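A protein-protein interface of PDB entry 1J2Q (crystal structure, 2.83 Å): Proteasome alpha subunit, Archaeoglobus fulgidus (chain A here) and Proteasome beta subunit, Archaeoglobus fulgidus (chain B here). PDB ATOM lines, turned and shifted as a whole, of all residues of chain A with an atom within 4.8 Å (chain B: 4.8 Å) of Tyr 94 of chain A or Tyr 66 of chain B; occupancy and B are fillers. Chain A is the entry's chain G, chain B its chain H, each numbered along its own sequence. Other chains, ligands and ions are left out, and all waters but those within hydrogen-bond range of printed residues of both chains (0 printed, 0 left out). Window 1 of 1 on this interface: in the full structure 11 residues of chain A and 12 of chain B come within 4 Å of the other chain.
The side-chain amide nitrogen (ND2) of Asn 90 of chain A lies within hydrogen-bond range of the backbone carbonyl oxygen (O) of Glu 96 of chain A (2.8 Å).
The backbone carbonyl oxygen (O) of Arg 77 of chain B is in hydrogen-bond range of the side-chain hydroxyl (OG1) of Thr 81 of chain B.
Of the 17 printed residues of chain B, 6 touch a printed residue of chain A.
Printed residues of chain B that touch a printed residue of chain A: Tyr 66, Arg 70, Arg 77, Ala 78, Thr 81 and Leu 82.
Of the 7 printed residues of chain A, 6 touch a printed residue of chain B.
Hydrophobic or aromatic side chains of chain A within 4 Å of the printed part of chain B: Tyr 94.
Tyr 94 of chain A touches five residues of chain B.
Printed residues of chain A within 4 Å of Tyr 66 of chain B: Tyr 94.
Of the printed residues of chain A, Ala 78 of chain B touches Tyr 94 (3.3 Å) and Glu 96 (3.8 Å).
Of the printed residues of chain A, Arg 77 of chain B touches Tyr 94 (3.9 Å), Asp 95 (3.4 Å) and Glu 96 (3.8 Å).
Of the printed residues of chain A, Arg 70 of chain B touches Asn 90 (3.0 Å) and Tyr 94 (3.4 Å).
Of the printed residues of chain B, Thr 93 of chain A touches Thr 81 (3.4 Å) and Leu 82 (3.4 Å).
Arg 91 of chain A touches none of the printed residues of chain B.
Glu 62 of chain B touches none of the printed residues of chain A.
The nearest residue of chain B that does not touch Tyr 94 of chain A is Leu 82 of chain B (4.1 Å).
The nearest residue of chain A that does not touch Tyr 66 of chain B is Glu 96 of chain A (4.3 Å).
The nearest printed residue of chain A that does not touch Arg 70 of chain B is Thr 93 of chain A (6.4 Å).
The backbone carbonyl oxygen (O) of Tyr 94 of chain A is in hydrogen-bond range of the side-chain hydroxyl (OG1) of Thr 81 of chain B (3.4 Å).
NH1 of Arg 70 of chain B lies within hydrogen-bond range of OD1 of Asn 90 of chain A.
N of Leu 82 of chain B is in hydrogen-bond range of O of Thr 93 of chain A.
OD1 of Asp 95 of chain A is in salt-bridge range of NH2 of Arg 77 of chain B, 3.7 Å away.
Among the printed residues, pairs that only touch across the chains: Leu 92 of chain A with Thr 81 of chain B, Thr 93 of chain A with Thr 81 of chain B, Tyr 94 of chain A with Tyr 66 of chain B, Tyr 94 of chain A with Arg 70 of chain B, Tyr 94 of chain A with Arg 77 of chain B, Tyr 94 of chain A with Ala 78 of chain B, Asp 95 of chain A with Thr 81 of chain B, Glu 96 of chain A with Arg 77 of chain B and Glu 96 of chain A with Ala 78 of chain B.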
ATOM      1  N   ASN A  90      -8.509  26.005  23.173  1.00  0.00           N
ATOM      2  CA  ASN A  90      -8.806  24.707  23.739  1.00  0.00           C
ATOM      3  C   ASN A  90      -7.519  23.991  24.145  1.00  0.00           C
ATOM      4  O   ASN A  90      -7.462  23.339  25.187  1.00  0.00           O
ATOM      5  CB  ASN A  90      -9.560  23.850  22.740  1.00  0.00           C
ATOM      6  CG  ASN A  90     -10.220  22.673  23.394  1.00  0.00           C
ATOM      7  OD1 ASN A  90     -11.272  22.818  24.011  1.00  0.00           O
ATOM      8  ND2 ASN A  90      -9.602  21.503  23.287  1.00  0.00           N
ATOM      9  N   ARG A  91      -6.495  24.098  23.305  1.00  0.00           N
ATOM     10  CA  ARG A  91      -5.210  23.467  23.584  1.00  0.00           C
ATOM     11  C   ARG A  91      -4.588  24.118  24.809  1.00  0.00           C
ATOM     12  O   ARG A  91      -4.108  23.443  25.716  1.00  0.00           O
ATOM     13  CB  ARG A  91      -4.257  23.638  22.395  1.00  0.00           C
ATOM     14  CG  ARG A  91      -4.463  22.674  21.258  1.00  0.00           C
ATOM     15  CD  ARG A  91      -3.635  23.080  20.032  1.00  0.00           C
ATOM     16  NE  ARG A  91      -3.223  21.906  19.265  1.00  0.00           N
ATOM     17  CZ  ARG A  91      -4.067  21.030  18.740  1.00  0.00           C
ATOM     18  NH1 ARG A  91      -3.605  19.986  18.069  1.00  0.00           N
ATOM     19  NH2 ARG A  91      -5.373  21.217  18.879  1.00  0.00           N
ATOM     20  N   LEU A  92      -4.601  25.446  24.816  1.00  0.00           N
ATOM     21  CA  LEU A  92      -4.032  26.224  25.907  1.00  0.00           C
ATOM     22  C   LEU A  92      -4.594  25.833  27.280  1.00  0.00           C
ATOM     23  O   LEU A  92      -3.858  25.770  28.258  1.00  0.00           O
ATOM     24  CB  LEU A  92      -4.292  27.714  25.651  1.00  0.00           C
ATOM     25  CG  LEU A  92      -3.407  28.759  26.338  1.00  0.00           C
ATOM     26  CD1 LEU A  92      -4.296  29.897  26.842  1.00  0.00           C
ATOM     27  CD2 LEU A  92      -2.617  28.129  27.473  1.00  0.00           C
ATOM     28  N   THR A  93      -5.895  25.557  27.344  1.00  0.00           N
ATOM     29  CA  THR A  93      -6.521  25.218  28.609  1.00  0.00           C
ATOM     30  C   THR A  93      -6.633  23.752  28.971  1.00  0.00           C
ATOM     31  O   THR A  93      -6.696  23.421  30.159  1.00  0.00           O
ATOM     32  CB  THR A  93      -7.923  25.860  28.732  1.00  0.00           C
ATOM     33  OG1 THR A  93      -8.857  24.883  29.205  1.00  0.00           O
ATOM     34  CG2 THR A  93      -8.375  26.449  27.421  1.00  0.00           C
ATOM     35  N   TYR A  94      -6.653  22.871  27.977  1.00  0.00           N
ATOM     36  CA  TYR A  94      -6.769  21.437  28.268  1.00  0.00           C
ATOM     37  C   TYR A  94      -5.605  20.639  27.721  1.00  0.00           C
ATOM     38  O   TYR A  94      -5.495  19.446  27.956  1.00  0.00           O
ATOM     39  CB  TYR A  94      -8.074  20.867  27.698  1.00  0.00           C
ATOM     40  CG  TYR A  94      -9.325  21.524  28.229  1.00  0.00           C
ATOM     41  CD1 TYR A  94      -9.664  21.438  29.583  1.00  0.00           C
ATOM     42  CD2 TYR A  94     -10.166  22.253  27.379  1.00  0.00           C
ATOM     43  CE1 TYR A  94     -10.815  22.068  30.080  1.00  0.00           C
ATOM     44  CE2 TYR A  94     -11.313  22.889  27.866  1.00  0.00           C
ATOM     45  CZ  TYR A  94     -11.631  22.793  29.217  1.00  0.00           C
ATOM     46  OH  TYR A  94     -12.745  23.444  29.706  1.00  0.00           O
ATOM     47  N   ASP A  95      -4.726  21.310  27.000  1.00  0.00           N
ATOM     48  CA  ASP A  95      -3.578  20.650  26.414  1.00  0.00           C
ATOM     49  C   ASP A  95      -4.059  19.556  25.482  1.00  0.00           C
ATOM     50  O   ASP A  95      -3.442  18.494  25.374  1.00  0.00           O
ATOM     51  CB  ASP A  95      -2.688  20.035  27.489  1.00  0.00           C
ATOM     52  CG  ASP A  95      -1.291  19.736  26.974  1.00  0.00           C
ATOM     53  OD1 ASP A  95      -0.661  18.798  27.498  1.00  0.00           O
ATOM     54  OD2 ASP A  95      -0.819  20.449  26.055  1.00  0.00           O
ATOM     55  N   GLU A  96      -5.177  19.813  24.816  1.00  0.00           N
ATOM     56  CA  GLU A  96      -5.732  18.849  23.886  1.00  0.00           C
ATOM     57  C   GLU A  96      -6.434  19.531  22.748  1.00  0.00           C
ATOM     58  O   GLU A  96      -6.998  20.609  22.918  1.00  0.00           O
ATOM     59  CB  GLU A  96      -6.705  17.943  24.596  1.00  0.00           C
ATOM     60  CG  GLU A  96      -6.066  17.252  25.728  1.00  0.00           C
ATOM     61  CD  GLU A  96      -6.848  16.076  26.146  1.00  0.00           C
ATOM     62  OE1 GLU A  96      -8.084  16.236  26.286  1.00  0.00           O
ATOM     63  OE2 GLU A  96      -6.234  15.000  26.336  1.00  0.00           O
ATOM     64  N   GLU B  62     -15.955  21.767  37.188  1.00  0.00           N
ATOM     65  CA  GLU B  62     -15.450  21.927  35.833  1.00  0.00           C
ATOM     66  C   GLU B  62     -15.326  20.625  35.072  1.00  0.00           C
ATOM     67  O   GLU B  62     -15.494  20.599  33.868  1.00  0.00           O
ATOM     68  CB  GLU B  62     -14.114  22.665  35.845  1.00  0.00           C
ATOM     69  CG  GLU B  62     -14.285  24.119  36.206  1.00  0.00           C
ATOM     70  CD  GLU B  62     -13.031  24.925  35.980  1.00  0.00           C
ATOM     71  OE1 GLU B  62     -13.059  26.143  36.249  1.00  0.00           O
ATOM     72  OE2 GLU B  62     -12.017  24.354  35.531  1.00  0.00           O
ATOM     73  N   ALA B  63     -15.033  19.539  35.767  1.00  0.00           N
ATOM     74  CA  ALA B  63     -14.924  18.264  35.084  1.00  0.00           C
ATOM     75  C   ALA B  63     -16.323  17.917  34.602  1.00  0.00           C
ATOM     76  O   ALA B  63     -16.519  17.539  33.441  1.00  0.00           O
ATOM     77  CB  ALA B  63     -14.410  17.199  36.034  1.00  0.00           C
ATOM     78  N   ASN B  64     -17.296  18.063  35.500  1.00  0.00           N
ATOM     79  CA  ASN B  64     -18.688  17.768  35.182  1.00  0.00           C
ATOM     80  C   ASN B  64     -19.129  18.519  33.953  1.00  0.00           C
ATOM     81  O   ASN B  64     -19.434  17.934  32.926  1.00  0.00           O
ATOM     82  CB  ASN B  64     -19.605  18.172  36.328  1.00  0.00           C
ATOM     83  CG  ASN B  64     -19.408  17.325  37.543  1.00  0.00           C
ATOM     84  OD1 ASN B  64     -18.854  16.221  37.449  1.00  0.00           O
ATOM     85  ND2 ASN B  64     -19.873  17.817  38.704  1.00  0.00           N
ATOM     86  N   LEU B  65     -19.163  19.834  34.088  1.00  0.00           N
ATOM     87  CA  LEU B  65     -19.583  20.713  33.025  1.00  0.00           C
ATOM     88  C   LEU B  65     -18.893  20.360  31.711  1.00  0.00           C
ATOM     89  O   LEU B  65     -19.505  20.413  30.648  1.00  0.00           O
ATOM     90  CB  LEU B  65     -19.291  22.161  33.429  1.00  0.00           C
ATOM     91  CG  LEU B  65     -19.801  23.258  32.494  1.00  0.00           C
ATOM     92  CD1 LEU B  65     -21.301  23.045  32.270  1.00  0.00           C
ATOM     93  CD2 LEU B  65     -19.533  24.627  33.095  1.00  0.00           C
ATOM     94  N   TYR B  66     -17.622  19.985  31.782  1.00  0.00           N
ATOM     95  CA  TYR B  66     -16.888  19.629  30.577  1.00  0.00           C
ATOM     96  C   TYR B  66     -17.625  18.505  29.847  1.00  0.00           C
ATOM     97  O   TYR B  66     -17.962  18.613  28.661  1.00  0.00           O
ATOM     98  CB  TYR B  66     -15.485  19.156  30.934  1.00  0.00           C
ATOM     99  CG  TYR B  66     -14.610  18.834  29.735  1.00  0.00           C
ATOM    100  CD1 TYR B  66     -13.820  19.821  29.126  1.00  0.00           C
ATOM    101  CD2 TYR B  66     -14.538  17.529  29.229  1.00  0.00           C
ATOM    102  CE1 TYR B  66     -12.975  19.509  28.065  1.00  0.00           C
ATOM    103  CE2 TYR B  66     -13.697  17.216  28.164  1.00  0.00           C
ATOM    104  CZ  TYR B  66     -12.921  18.209  27.593  1.00  0.00           C
ATOM    105  OH  TYR B  66     -12.074  17.894  26.554  1.00  0.00           O
ATOM    106  N   GLU B  67     -17.866  17.421  30.580  1.00  0.00           N
ATOM    107  CA  GLU B  67     -18.553  16.265  30.036  1.00  0.00           C
ATOM    108  C   GLU B  67     -19.980  16.593  29.584  1.00  0.00           C
ATOM    109  O   GLU B  67     -20.340  16.335  28.438  1.00  0.00           O
ATOM    110  CB  GLU B  67     -18.581  15.146  31.072  1.00  0.00           C
ATOM    111  CG  GLU B  67     -19.253  13.897  30.570  1.00  0.00           C
ATOM    112  CD  GLU B  67     -19.551  12.926  31.680  1.00  0.00           C
ATOM    113  OE1 GLU B  67     -20.088  13.383  32.719  1.00  0.00           O
ATOM    114  OE2 GLU B  67     -19.264  11.714  31.513  1.00  0.00           O
ATOM    115  N   ILE B  68     -20.788  17.152  30.479  1.00  0.00           N
ATOM    116  CA  ILE B  68     -22.157  17.503  30.145  1.00  0.00           C
ATOM    117  C   ILE B  68     -22.198  18.313  28.845  1.00  0.00           C
ATOM    118  O   ILE B  68     -23.070  18.099  28.001  1.00  0.00           O
ATOM    119  CB  ILE B  68     -22.834  18.327  31.290  1.00  0.00           C
ATOM    120  CG1 ILE B  68     -23.250  17.420  32.452  1.00  0.00           C
ATOM    121  CG2 ILE B  68     -24.084  19.006  30.785  1.00  0.00           C
ATOM    122  CD1 ILE B  68     -22.105  16.736  33.193  1.00  0.00           C
ATOM    123  N   ARG B  69     -21.249  19.226  28.663  1.00  0.00           N
ATOM    124  CA  ARG B  69     -21.246  20.052  27.462  1.00  0.00           C
ATOM    125  C   ARG B  69     -20.700  19.399  26.209  1.00  0.00           C
ATOM    126  O   ARG B  69     -21.283  19.532  25.138  1.00  0.00           O
ATOM    127  CB  ARG B  69     -20.493  21.361  27.717  1.00  0.00           C
ATOM    128  CG  ARG B  69     -21.160  22.237  28.770  1.00  0.00           C
ATOM    129  CD  ARG B  69     -20.842  23.713  28.595  1.00  0.00           C
ATOM    130  NE  ARG B  69     -19.542  24.085  29.136  1.00  0.00           N
ATOM    131  CZ  ARG B  69     -19.278  25.262  29.698  1.00  0.00           C
ATOM    132  NH1 ARG B  69     -18.068  25.510  30.168  1.00  0.00           N
ATOM    133  NH2 ARG B  69     -20.225  26.190  29.801  1.00  0.00           N
ATOM    134  N   ARG B  70     -19.597  18.680  26.330  1.00  0.00           N
ATOM    135  CA  ARG B  70     -18.989  18.059  25.163  1.00  0.00           C
ATOM    136  C   ARG B  70     -19.326  16.591  25.011  1.00  0.00           C
ATOM    137  O   ARG B  70     -18.835  15.920  24.104  1.00  0.00           O
ATOM    138  CB  ARG B  70     -17.475  18.229  25.237  1.00  0.00           C
ATOM    139  CG  ARG B  70     -17.077  19.677  25.465  1.00  0.00           C
ATOM    140  CD  ARG B  70     -15.666  19.815  26.006  1.00  0.00           C
ATOM    141  NE  ARG B  70     -15.434  21.176  26.490  1.00  0.00           N
ATOM    142  CZ  ARG B  70     -14.571  22.014  25.942  1.00  0.00           C
ATOM    143  NH1 ARG B  70     -13.854  21.627  24.891  1.00  0.00           N
ATOM    144  NH2 ARG B  70     -14.431  23.229  26.453  1.00  0.00           N
ATOM    145  N   GLU B  71     -20.160  16.090  25.908  1.00  0.00           N
ATOM    146  CA  GLU B  71     -20.565  14.691  25.877  1.00  0.00           C
ATOM    147  C   GLU B  71     -19.379  13.729  25.802  1.00  0.00           C
ATOM    148  O   GLU B  71     -19.498  12.625  25.282  1.00  0.00           O
ATOM    149  CB  GLU B  71     -21.523  14.456  24.709  1.00  0.00           C
ATOM    150  CG  GLU B  71     -22.712  15.419  24.703  1.00  0.00           C
ATOM    151  CD  GLU B  71     -23.767  15.056  23.672  1.00  0.00           C
ATOM    152  OE1 GLU B  71     -24.475  14.050  23.885  1.00  0.00           O
ATOM    153  OE2 GLU B  71     -23.884  15.774  22.652  1.00  0.00           O
ATOM    154  N   ARG B  72     -18.234  14.170  26.312  1.00  0.00           N
ATOM    155  CA  ARG B  72     -17.030  13.343  26.365  1.00  0.00           C
ATOM    156  C   ARG B  72     -16.512  13.538  27.767  1.00  0.00           C
ATOM    157  O   ARG B  72     -16.696  14.598  28.355  1.00  0.00           O
ATOM    158  CB  ARG B  72     -15.935  13.822  25.410  1.00  0.00           C
ATOM    159  CG  ARG B  72     -16.278  13.840  23.953  1.00  0.00           C
ATOM    160  CD  ARG B  72     -15.042  14.218  23.153  1.00  0.00           C
ATOM    161  NE  ARG B  72     -14.004  13.196  23.254  1.00  0.00           N
ATOM    162  CZ  ARG B  72     -13.096  12.956  22.306  1.00  0.00           C
ATOM    163  NH1 ARG B  72     -12.184  12.004  22.475  1.00  0.00           N
ATOM    164  NH2 ARG B  72     -13.097  13.661  21.179  1.00  0.00           N
ATOM    165  N   LYS B  73     -15.873  12.519  28.316  1.00  0.00           N
ATOM    166  CA  LYS B  73     -15.314  12.656  29.644  1.00  0.00           C
ATOM    167  C   LYS B  73     -13.978  13.351  29.463  1.00  0.00           C
ATOM    168  O   LYS B  73     -13.291  13.139  28.464  1.00  0.00           O
ATOM    169  CB  LYS B  73     -15.118  11.290  30.289  1.00  0.00           C
ATOM    170  CG  LYS B  73     -16.419  10.659  30.702  1.00  0.00           C
ATOM    171  CD  LYS B  73     -16.202   9.310  31.344  1.00  0.00           C
ATOM    172  CE  LYS B  73     -17.514   8.754  31.867  1.00  0.00           C
ATOM    173  NZ  LYS B  73     -17.307   7.400  32.466  1.00  0.00           N
ATOM    174  N   PRO B  74     -13.608  14.217  30.411  1.00  0.00           N
ATOM    175  CA  PRO B  74     -12.325  14.902  30.268  1.00  0.00           C
ATOM    176  C   PRO B  74     -11.173  13.956  30.606  1.00  0.00           C
ATOM    177  O   PRO B  74     -11.279  13.124  31.502  1.00  0.00           O
ATOM    178  CB  PRO B  74     -12.453  16.070  31.244  1.00  0.00           C
ATOM    179  CG  PRO B  74     -13.318  15.500  32.338  1.00  0.00           C
ATOM    180  CD  PRO B  74     -14.362  14.718  31.576  1.00  0.00           C
ATOM    181  N   ARG B  77      -5.217  14.447  31.543  1.00  0.00           N
ATOM    182  CA  ARG B  77      -4.351  15.492  31.028  1.00  0.00           C
ATOM    183  C   ARG B  77      -5.091  16.828  31.011  1.00  0.00           C
ATOM    184  O   ARG B  77      -4.544  17.862  31.405  1.00  0.00           O
ATOM    185  CB  ARG B  77      -3.883  15.155  29.613  1.00  0.00           C
ATOM    186  CG  ARG B  77      -3.030  16.239  28.980  1.00  0.00           C
ATOM    187  CD  ARG B  77      -2.746  15.963  27.502  1.00  0.00           C
ATOM    188  NE  ARG B  77      -2.079  14.678  27.312  1.00  0.00           N
ATOM    189  CZ  ARG B  77      -0.867  14.383  27.783  1.00  0.00           C
ATOM    190  NH1 ARG B  77      -0.337  13.178  27.575  1.00  0.00           N
ATOM    191  NH2 ARG B  77      -0.173  15.298  28.459  1.00  0.00           N
ATOM    192  N   ALA B  78      -6.338  16.804  30.553  1.00  0.00           N
ATOM    193  CA  ALA B  78      -7.141  18.018  30.476  1.00  0.00           C
ATOM    194  C   ALA B  78      -7.364  18.633  31.856  1.00  0.00           C
ATOM    195  O   ALA B  78      -7.175  19.842  32.053  1.00  0.00           O
ATOM    196  CB  ALA B  78      -8.480  17.715  29.814  1.00  0.00           C
ATOM    197  N   THR B  81      -4.064  20.006  33.203  1.00  0.00           N
ATOM    198  CA  THR B  81      -3.676  21.233  32.516  1.00  0.00           C
ATOM    199  C   THR B  81      -4.545  22.371  33.045  1.00  0.00           C
ATOM    200  O   THR B  81      -4.080  23.487  33.308  1.00  0.00           O
ATOM    201  CB  THR B  81      -3.931  21.122  30.988  1.00  0.00           C
ATOM    202  OG1 THR B  81      -3.272  19.958  30.464  1.00  0.00           O
ATOM    203  CG2 THR B  81      -3.418  22.363  30.269  1.00  0.00           C
ATOM    204  N   LEU B  82      -5.829  22.070  33.168  1.00  0.00           N
ATOM    205  CA  LEU B  82      -6.799  23.023  33.669  1.00  0.00           C
ATOM    206  C   LEU B  82      -6.350  23.519  35.043  1.00  0.00           C
ATOM    207  O   LEU B  82      -6.202  24.715  35.258  1.00  0.00           O
ATOM    208  CB  LEU B  82      -8.141  22.324  33.778  1.00  0.00           C
ATOM    209  CG  LEU B  82      -9.303  23.116  34.336  1.00  0.00           C
ATOM    210  CD1 LEU B  82      -9.689  24.247  33.363  1.00  0.00           C
ATOM    211  CD2 LEU B  82     -10.454  22.157  34.557  1.00  0.00           C
